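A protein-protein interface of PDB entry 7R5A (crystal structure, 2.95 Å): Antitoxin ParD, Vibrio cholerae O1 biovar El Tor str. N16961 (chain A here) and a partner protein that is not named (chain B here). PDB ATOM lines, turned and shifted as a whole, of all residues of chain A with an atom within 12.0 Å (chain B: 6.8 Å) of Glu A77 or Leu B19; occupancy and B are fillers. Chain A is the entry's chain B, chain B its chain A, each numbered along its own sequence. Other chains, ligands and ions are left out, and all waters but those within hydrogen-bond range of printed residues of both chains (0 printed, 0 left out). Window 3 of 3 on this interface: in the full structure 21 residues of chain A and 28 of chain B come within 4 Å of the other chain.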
ATOM      1  N   TYR A  65      21.366  21.320  37.911  1.00  0.00           N
ATOM      2  CA  TYR A  65      20.368  22.070  37.162  1.00  0.00           C
ATOM      3  C   TYR A  65      19.418  22.794  38.104  1.00  0.00           C
ATOM      4  O   TYR A  65      18.889  22.199  39.047  1.00  0.00           O
ATOM      5  CB  TYR A  65      19.564  21.158  36.227  1.00  0.00           C
ATOM      6  CG  TYR A  65      18.383  21.856  35.584  1.00  0.00           C
ATOM      7  CD1 TYR A  65      18.560  22.711  34.502  1.00  0.00           C
ATOM      8  CD2 TYR A  65      17.092  21.667  36.063  1.00  0.00           C
ATOM      9  CE1 TYR A  65      17.486  23.353  33.916  1.00  0.00           C
ATOM     10  CE2 TYR A  65      16.013  22.305  35.483  1.00  0.00           C
ATOM     11  CZ  TYR A  65      16.216  23.146  34.410  1.00  0.00           C
ATOM     12  OH  TYR A  65      15.143  23.783  33.829  1.00  0.00           O
ATOM     13  N   ASP A  68      16.313  28.989  37.273  1.00  0.00           N
ATOM     14  CA  ASP A  68      16.765  30.376  37.310  1.00  0.00           C
ATOM     15  C   ASP A  68      18.280  30.478  37.186  1.00  0.00           C
ATOM     16  O   ASP A  68      18.793  31.410  36.554  1.00  0.00           O
ATOM     17  CB  ASP A  68      16.271  31.052  38.586  1.00  0.00           C
ATOM     18  CG  ASP A  68      14.768  31.266  38.582  1.00  0.00           C
ATOM     19  OD1 ASP A  68      14.207  31.526  37.494  1.00  0.00           O
ATOM     20  OD2 ASP A  68      14.148  31.181  39.666  1.00  0.00           O
ATOM     21  N   SER A  69      19.017  29.526  37.765  1.00  0.00           N
ATOM     22  CA  SER A  69      20.468  29.512  37.590  1.00  0.00           C
ATOM     23  C   SER A  69      20.846  29.236  36.139  1.00  0.00           C
ATOM     24  O   SER A  69      21.796  29.830  35.612  1.00  0.00           O
ATOM     25  CB  SER A  69      21.098  28.473  38.517  1.00  0.00           C
ATOM     26  OG  SER A  69      20.807  28.762  39.873  1.00  0.00           O
ATOM     27  N   PHE A  70      20.109  28.339  35.479  1.00  0.00           N
ATOM     28  CA  PHE A  70      20.330  28.075  34.061  1.00  0.00           C
ATOM     29  C   PHE A  70      20.075  29.323  33.224  1.00  0.00           C
ATOM     30  O   PHE A  70      20.845  29.639  32.307  1.00  0.00           O
ATOM     31  CB  PHE A  70      19.427  26.923  33.618  1.00  0.00           C
ATOM     32  CG  PHE A  70      19.708  26.415  32.236  1.00  0.00           C
ATOM     33  CD1 PHE A  70      20.940  25.869  31.922  1.00  0.00           C
ATOM     34  CD2 PHE A  70      18.727  26.455  31.259  1.00  0.00           C
ATOM     35  CE1 PHE A  70      21.197  25.391  30.653  1.00  0.00           C
ATOM     36  CE2 PHE A  70      18.977  25.977  29.989  1.00  0.00           C
ATOM     37  CZ  PHE A  70      20.213  25.444  29.685  1.00  0.00           C
ATOM     38  N   ILE A  71      19.000  30.050  33.532  1.00  0.00           N
ATOM     39  CA  ILE A  71      18.694  31.278  32.804  1.00  0.00           C
ATOM     40  C   ILE A  71      19.767  32.333  33.052  1.00  0.00           C
ATOM     41  O   ILE A  71      20.162  33.060  32.134  1.00  0.00           O
ATOM     42  CB  ILE A  71      17.291  31.785  33.185  1.00  0.00           C
ATOM     43  CG1 ILE A  71      16.230  30.763  32.774  1.00  0.00           C
ATOM     44  CG2 ILE A  71      17.008  33.130  32.536  1.00  0.00           C
ATOM     45  CD1 ILE A  71      14.819  31.159  33.150  1.00  0.00           C
ATOM     46  N   ASN A  72      20.262  32.432  34.290  1.00  0.00           N
ATOM     47  CA  ASN A  72      21.330  33.383  34.588  1.00  0.00           C
ATOM     48  C   ASN A  72      22.603  33.039  33.824  1.00  0.00           C
ATOM     49  O   ASN A  72      23.294  33.931  33.319  1.00  0.00           O
ATOM     50  CB  ASN A  72      21.602  33.419  36.092  1.00  0.00           C
ATOM     51  CG  ASN A  72      20.505  34.118  36.869  1.00  0.00           C
ATOM     52  OD1 ASN A  72      19.851  35.030  36.361  1.00  0.00           O
ATOM     53  ND2 ASN A  72      20.299  33.696  38.111  1.00  0.00           N
ATOM     54  N   GLU A  73      22.928  31.749  33.728  1.00  0.00           N
ATOM     55  CA  GLU A  73      24.091  31.331  32.953  1.00  0.00           C
ATOM     56  C   GLU A  73      23.922  31.689  31.479  1.00  0.00           C
ATOM     57  O   GLU A  73      24.835  32.241  30.848  1.00  0.00           O
ATOM     58  CB  GLU A  73      24.310  29.827  33.138  1.00  0.00           C
ATOM     59  CG  GLU A  73      25.611  29.281  32.574  1.00  0.00           C
ATOM     60  CD  GLU A  73      25.503  28.906  31.110  1.00  0.00           C
ATOM     61  OE1 GLU A  73      25.979  29.688  30.264  1.00  0.00           O
ATOM     62  OE2 GLU A  73      24.935  27.835  30.806  1.00  0.00           O
ATOM     63  N   LEU A  74      22.744  31.398  30.918  1.00  0.00           N
ATOM     64  CA  LEU A  74      22.485  31.723  29.518  1.00  0.00           C
ATOM     65  C   LEU A  74      22.556  33.226  29.270  1.00  0.00           C
ATOM     66  O   LEU A  74      23.000  33.664  28.202  1.00  0.00           O
ATOM     67  CB  LEU A  74      21.122  31.178  29.096  1.00  0.00           C
ATOM     68  CG  LEU A  74      21.004  29.654  29.069  1.00  0.00           C
ATOM     69  CD1 LEU A  74      19.608  29.236  28.651  1.00  0.00           C
ATOM     70  CD2 LEU A  74      22.047  29.065  28.137  1.00  0.00           C
ATOM     71  N   ASP A  75      22.118  34.030  30.241  1.00  0.00           N
ATOM     72  CA  ASP A  75      22.215  35.479  30.096  1.00  0.00           C
ATOM     73  C   ASP A  75      23.661  35.944  30.196  1.00  0.00           C
ATOM     74  O   ASP A  75      24.065  36.889  29.508  1.00  0.00           O
ATOM     75  CB  ASP A  75      21.357  36.177  31.151  1.00  0.00           C
ATOM     76  CG  ASP A  75      19.878  35.895  30.982  1.00  0.00           C
ATOM     77  OD1 ASP A  75      19.527  35.058  30.125  1.00  0.00           O
ATOM     78  OD2 ASP A  75      19.067  36.514  31.703  1.00  0.00           O
ATOM     79  N   SER A  76      24.454  35.295  31.052  1.00  0.00           N
ATOM     80  CA  SER A  76      25.861  35.648  31.176  1.00  0.00           C
ATOM     81  C   SER A  76      26.662  35.257  29.943  1.00  0.00           C
ATOM     82  O   SER A  76      27.719  35.849  29.695  1.00  0.00           O
ATOM     83  CB  SER A  76      26.468  34.987  32.415  1.00  0.00           C
ATOM     84  OG  SER A  76      26.617  33.591  32.227  1.00  0.00           O
ATOM     85  N   GLU A  77      26.195  34.275  29.173  1.00  0.00           N
ATOM     86  CA  GLU A  77      26.881  33.913  27.936  1.00  0.00           C
ATOM     87  C   GLU A  77      26.924  35.083  26.958  1.00  0.00           C
ATOM     88  O   GLU A  77      28.003  35.607  26.664  1.00  0.00           O
ATOM     89  CB  GLU A  77      26.216  32.702  27.281  1.00  0.00           C
ATOM     90  CG  GLU A  77      26.754  31.372  27.775  1.00  0.00           C
ATOM     91  CD  GLU A  77      26.246  30.200  26.960  1.00  0.00           C
ATOM     92  OE1 GLU A  77      25.748  30.429  25.837  1.00  0.00           O
ATOM     93  OE2 GLU A  77      26.345  29.051  27.438  1.00  0.00           O
ATOM     94  N   ASN A  78      25.768  35.496  26.447  1.00  0.00           N
ATOM     95  CA  ASN A  78      25.711  36.632  25.532  1.00  0.00           C
ATOM     96  C   ASN A  78      25.992  37.936  26.269  1.00  0.00           C
ATOM     97  O   ASN A  78      27.144  38.346  26.403  1.00  0.00           O
ATOM     98  CB  ASN A  78      24.352  36.708  24.833  1.00  0.00           C
ATOM     99  CG  ASN A  78      24.281  35.834  23.598  1.00  0.00           C
ATOM    100  OD1 ASN A  78      24.935  34.793  23.518  1.00  0.00           O
ATOM    101  ND2 ASN A  78      23.490  36.258  22.618  1.00  0.00           N
ATOM    102  N   LEU B  14      19.139  20.929  26.410  1.00  0.00           N
ATOM    103  CA  LEU B  14      18.291  22.044  26.814  1.00  0.00           C
ATOM    104  C   LEU B  14      18.935  23.377  26.457  1.00  0.00           C
ATOM    105  O   LEU B  14      18.248  24.309  26.022  1.00  0.00           O
ATOM    106  CB  LEU B  14      17.997  21.968  28.312  1.00  0.00           C
ATOM    107  CG  LEU B  14      16.914  22.912  28.839  1.00  0.00           C
ATOM    108  CD1 LEU B  14      15.605  22.684  28.101  1.00  0.00           C
ATOM    109  CD2 LEU B  14      16.724  22.729  30.337  1.00  0.00           C
ATOM    110  N   ARG B  15      20.257  23.483  26.616  1.00  0.00           N
ATOM    111  CA  ARG B  15      20.954  24.709  26.238  1.00  0.00           C
ATOM    112  C   ARG B  15      20.883  24.943  24.735  1.00  0.00           C
ATOM    113  O   ARG B  15      20.696  26.080  24.287  1.00  0.00           O
ATOM    114  CB  ARG B  15      22.410  24.651  26.701  1.00  0.00           C
ATOM    115  CG  ARG B  15      23.140  25.979  26.583  1.00  0.00           C
ATOM    116  CD  ARG B  15      24.575  25.885  27.074  1.00  0.00           C
ATOM    117  NE  ARG B  15      25.494  25.476  26.015  1.00  0.00           N
ATOM    118  CZ  ARG B  15      26.099  26.324  25.191  1.00  0.00           C
ATOM    119  NH1 ARG B  15      25.880  27.627  25.302  1.00  0.00           N
ATOM    120  NH2 ARG B  15      26.922  25.872  24.253  1.00  0.00           N
ATOM    121  N   ASP B  16      21.038  23.880  23.942  1.00  0.00           N
ATOM    122  CA  ASP B  16      20.907  24.003  22.494  1.00  0.00           C
ATOM    123  C   ASP B  16      19.526  24.519  22.117  1.00  0.00           C
ATOM    124  O   ASP B  16      19.394  25.445  21.307  1.00  0.00           O
ATOM    125  CB  ASP B  16      21.173  22.655  21.824  1.00  0.00           C
ATOM    126  CG  ASP B  16      22.637  22.271  21.848  1.00  0.00           C
ATOM    127  OD1 ASP B  16      23.467  23.129  22.209  1.00  0.00           O
ATOM    128  OD2 ASP B  16      22.957  21.113  21.507  1.00  0.00           O
ATOM    129  N   ILE B  17      18.480  23.931  22.699  1.00  0.00           N
ATOM    130  CA  ILE B  17      17.122  24.348  22.359  1.00  0.00           C
ATOM    131  C   ILE B  17      16.879  25.787  22.797  1.00  0.00           C
ATOM    132  O   ILE B  17      16.240  26.570  22.080  1.00  0.00           O
ATOM    133  CB  ILE B  17      16.090  23.387  22.976  1.00  0.00           C
ATOM    134  CG1 ILE B  17      16.419  21.939  22.619  1.00  0.00           C
ATOM    135  CG2 ILE B  17      14.706  23.712  22.460  1.00  0.00           C
ATOM    136  CD1 ILE B  17      15.667  20.924  23.453  1.00  0.00           C
ATOM    137  N   ALA B  18      17.390  26.163  23.973  1.00  0.00           N
ATOM    138  CA  ALA B  18      17.208  27.525  24.461  1.00  0.00           C
ATOM    139  C   ALA B  18      17.890  28.529  23.543  1.00  0.00           C
ATOM    140  O   ALA B  18      17.298  29.550  23.174  1.00  0.00           O
ATOM    141  CB  ALA B  18      17.742  27.643  25.888  1.00  0.00           C
ATOM    142  N   LEU B  19      19.137  28.251  23.154  1.00  0.00           N
ATOM    143  CA  LEU B  19      19.848  29.159  22.260  1.00  0.00           C
ATOM    144  C   LEU B  19      19.172  29.236  20.899  1.00  0.00           C
ATOM    145  O   LEU B  19      19.114  30.309  20.288  1.00  0.00           O
ATOM    146  CB  LEU B  19      21.305  28.724  22.112  1.00  0.00           C
ATOM    147  CG  LEU B  19      22.210  28.956  23.323  1.00  0.00           C
ATOM    148  CD1 LEU B  19      23.647  28.596  22.987  1.00  0.00           C
ATOM    149  CD2 LEU B  19      22.107  30.398  23.798  1.00  0.00           C
ATOM    150  N   PHE B  20      18.639  28.113  20.412  1.00  0.00           N
ATOM    151  CA  PHE B  20      17.951  28.119  19.125  1.00  0.00           C
ATOM    152  C   PHE B  20      16.705  28.996  19.175  1.00  0.00           C
ATOM    153  O   PHE B  20      16.523  29.889  18.336  1.00  0.00           O
ATOM    154  CB  PHE B  20      17.596  26.688  18.720  1.00  0.00           C
ATOM    155  CG  PHE B  20      16.664  26.602  17.548  1.00  0.00           C
ATOM    156  CD1 PHE B  20      17.059  27.043  16.297  1.00  0.00           C
ATOM    157  CD2 PHE B  20      15.395  26.066  17.695  1.00  0.00           C
ATOM    158  CE1 PHE B  20      16.201  26.962  15.215  1.00  0.00           C
ATOM    159  CE2 PHE B  20      14.534  25.980  16.617  1.00  0.00           C
ATOM    160  CZ  PHE B  20      14.938  26.429  15.375  1.00  0.00           C
ATOM    161  N   THR B  21      15.839  28.765  20.166  1.00  0.00           N
ATOM    162  CA  THR B  21      14.625  29.562  20.283  1.00  0.00           C
ATOM    163  C   THR B  21      14.917  31.018  20.627  1.00  0.00           C
ATOM    164  O   THR B  21      14.090  31.888  20.333  1.00  0.00           O
ATOM    165  CB  THR B  21      13.687  28.958  21.330  1.00  0.00           C
ATOM    166  OG1 THR B  21      14.340  28.931  22.604  1.00  0.00           O
ATOM    167  CG2 THR B  21      13.292  27.540  20.937  1.00  0.00           C
ATOM    168  N   GLN B  22      16.071  31.307  21.235  1.00  0.00           N
ATOM    169  CA  GLN B  22      16.440  32.693  21.495  1.00  0.00           C
ATOM    170  C   GLN B  22      16.920  33.388  20.228  1.00  0.00           C
ATOM    171  O   GLN B  22      16.543  34.535  19.965  1.00  0.00           O
ATOM    172  CB  GLN B  22      17.518  32.755  22.580  1.00  0.00           C
ATOM    173  CG  GLN B  22      18.023  34.161  22.883  1.00  0.00           C
ATOM    174  CD  GLN B  22      19.166  34.173  23.883  1.00  0.00           C
ATOM    175  OE1 GLN B  22      19.565  33.129  24.399  1.00  0.00           O
ATOM    176  NE2 GLN B  22      19.699  35.357  24.159  1.00  0.00           N
ATOM    177  N   ARG B  23      17.749  32.709  19.432  1.00  0.00           N
ATOM    178  CA  ARG B  23      18.227  33.300  18.188  1.00  0.00           C
ATOM    179  C   ARG B  23      17.109  33.428  17.162  1.00  0.00           C
ATOM    180  O   ARG B  23      17.185  34.283  16.272  1.00  0.00           O
ATOM    181  CB  ARG B  23      19.376  32.469  17.617  1.00  0.00           C
ATOM    182  N   ARG B  24      16.070  32.599  17.263  1.00  0.00           N
ATOM    183  CA  ARG B  24      14.977  32.681  16.299  1.00  0.00           C
ATOM    184  C   ARG B  24      13.875  33.637  16.746  1.00  0.00           C
ATOM    185  O   ARG B  24      13.418  34.470  15.957  1.00  0.00           O
ATOM    186  CB  ARG B  24      14.392  31.289  16.042  1.00  0.00           C
ATOM    187  CG  ARG B  24      13.276  31.275  15.007  1.00  0.00           C
ATOM    188  CD  ARG B  24      12.806  29.859  14.702  1.00  0.00           C
ATOM    189  NE  ARG B  24      11.759  29.837  13.683  1.00  0.00           N
ATOM    190  CZ  ARG B  24      11.209  28.727  13.199  1.00  0.00           C
ATOM    191  NH1 ARG B  24      10.263  28.805  12.272  1.00  0.00           N
ATOM    192  NH2 ARG B  24      11.605  27.541  13.639  1.00  0.00           N
ATOM    193  N   ARG B  30      12.543  32.534  24.972  1.00  0.00           N
ATOM    194  CA  ARG B  30      13.390  31.482  25.524  1.00  0.00           C
ATOM    195  C   ARG B  30      13.089  31.250  26.998  1.00  0.00           C
ATOM    196  O   ARG B  30      13.067  30.104  27.462  1.00  0.00           O
ATOM    197  CB  ARG B  30      14.860  31.845  25.329  1.00  0.00           C
ATOM    198  CG  ARG B  30      15.835  30.864  25.950  1.00  0.00           C
ATOM    199  CD  ARG B  30      17.127  31.564  26.322  1.00  0.00           C
ATOM    200  NE  ARG B  30      16.929  32.507  27.419  1.00  0.00           N
ATOM    201  CZ  ARG B  30      17.798  33.452  27.759  1.00  0.00           C
ATOM    202  NH1 ARG B  30      18.929  33.593  27.080  1.00  0.00           N
ATOM    203  NH2 ARG B  30      17.535  34.263  28.775  1.00  0.00           N
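NH1 of Arg B15 lies within salt-bridge range of OE2 of Glu A77, at 2.6 Å.
The guanidinium group of Arg B30 is in salt-bridge range of the side-chain carboxylate of Asp A75, 2.5 Å away.
The side-chain amide oxygen (OE1) of Gln B22 lies within hydrogen-bond range of the guanidinium group (NH1) of Arg B30 (2.8 Å).
The backbone carbonyl oxygen (O) of Ala B18 sits at hydrogen-bond distance from the side-chain hydroxyl (OG1) of Thr B21, 3.1 Å away.
Tyr A65 touches Leu B14 (CE1 to CD2, 3.7 Å).
Leu B14 touches Phe A70 (CG to CE2, 3.9 Å).
Phe A70 touches Arg B15 (CZ to CA, 3.6 Å).
Ile A71 touches Arg B30.
Arg B15 touches Leu A74 (CG to CD2, 3.6 Å).
CB of Ala B18 touches CD1 of Leu A74, at 3.7 Å.
CB of Leu A74 touches NH1 of Arg B30, at 3.8 Å.
Leu B19 touches Glu A77 (CD1 to OE1, 3.99 Å).
Printed residues of chain A within 4 Å of Leu B19: Glu A77.
Arg B15 touches three residues of chain A.
No residue of chain A comes within 4 Å of Phe B20.
No residue of chain A comes within 4 Å of Arg B23.
Of the printed residues of chain A, Arg B30 touches Ile A71 (3.96 Å), Leu A74 (3.8 Å) and Asp A75 (2.5 Å).
Of the printed residues of chain B, Asp A75 touches Arg B30.
Asn A72 touches none of the printed residues of chain B.
Ser A76 touches none of the printed residues of chain B.
The nearest printed residue of chain B that does not touch Tyr A65 is Arg B15 (7.8 Å).
Of the 12 printed residues of chain A, 6 touch a printed residue of chain B.
Hydrophobic or aromatic side chains of chain A that line the printed part of chain B: Tyr A65, Phe A70, Ile A71 and Leu A74.
Hydrophobic or aromatic side chains of chain B within 4 Å of the printed part of chain A: Leu B14, Ala B18 and Leu B19.
Among the printed residues, Asp or Glu carboxylates within 4 Å of a Lys or Arg side-chain nitrogen of the other chain: Asp A75 with Arg B30 (2.5 Å) and Glu A77 with Arg B15 (2.6 Å).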
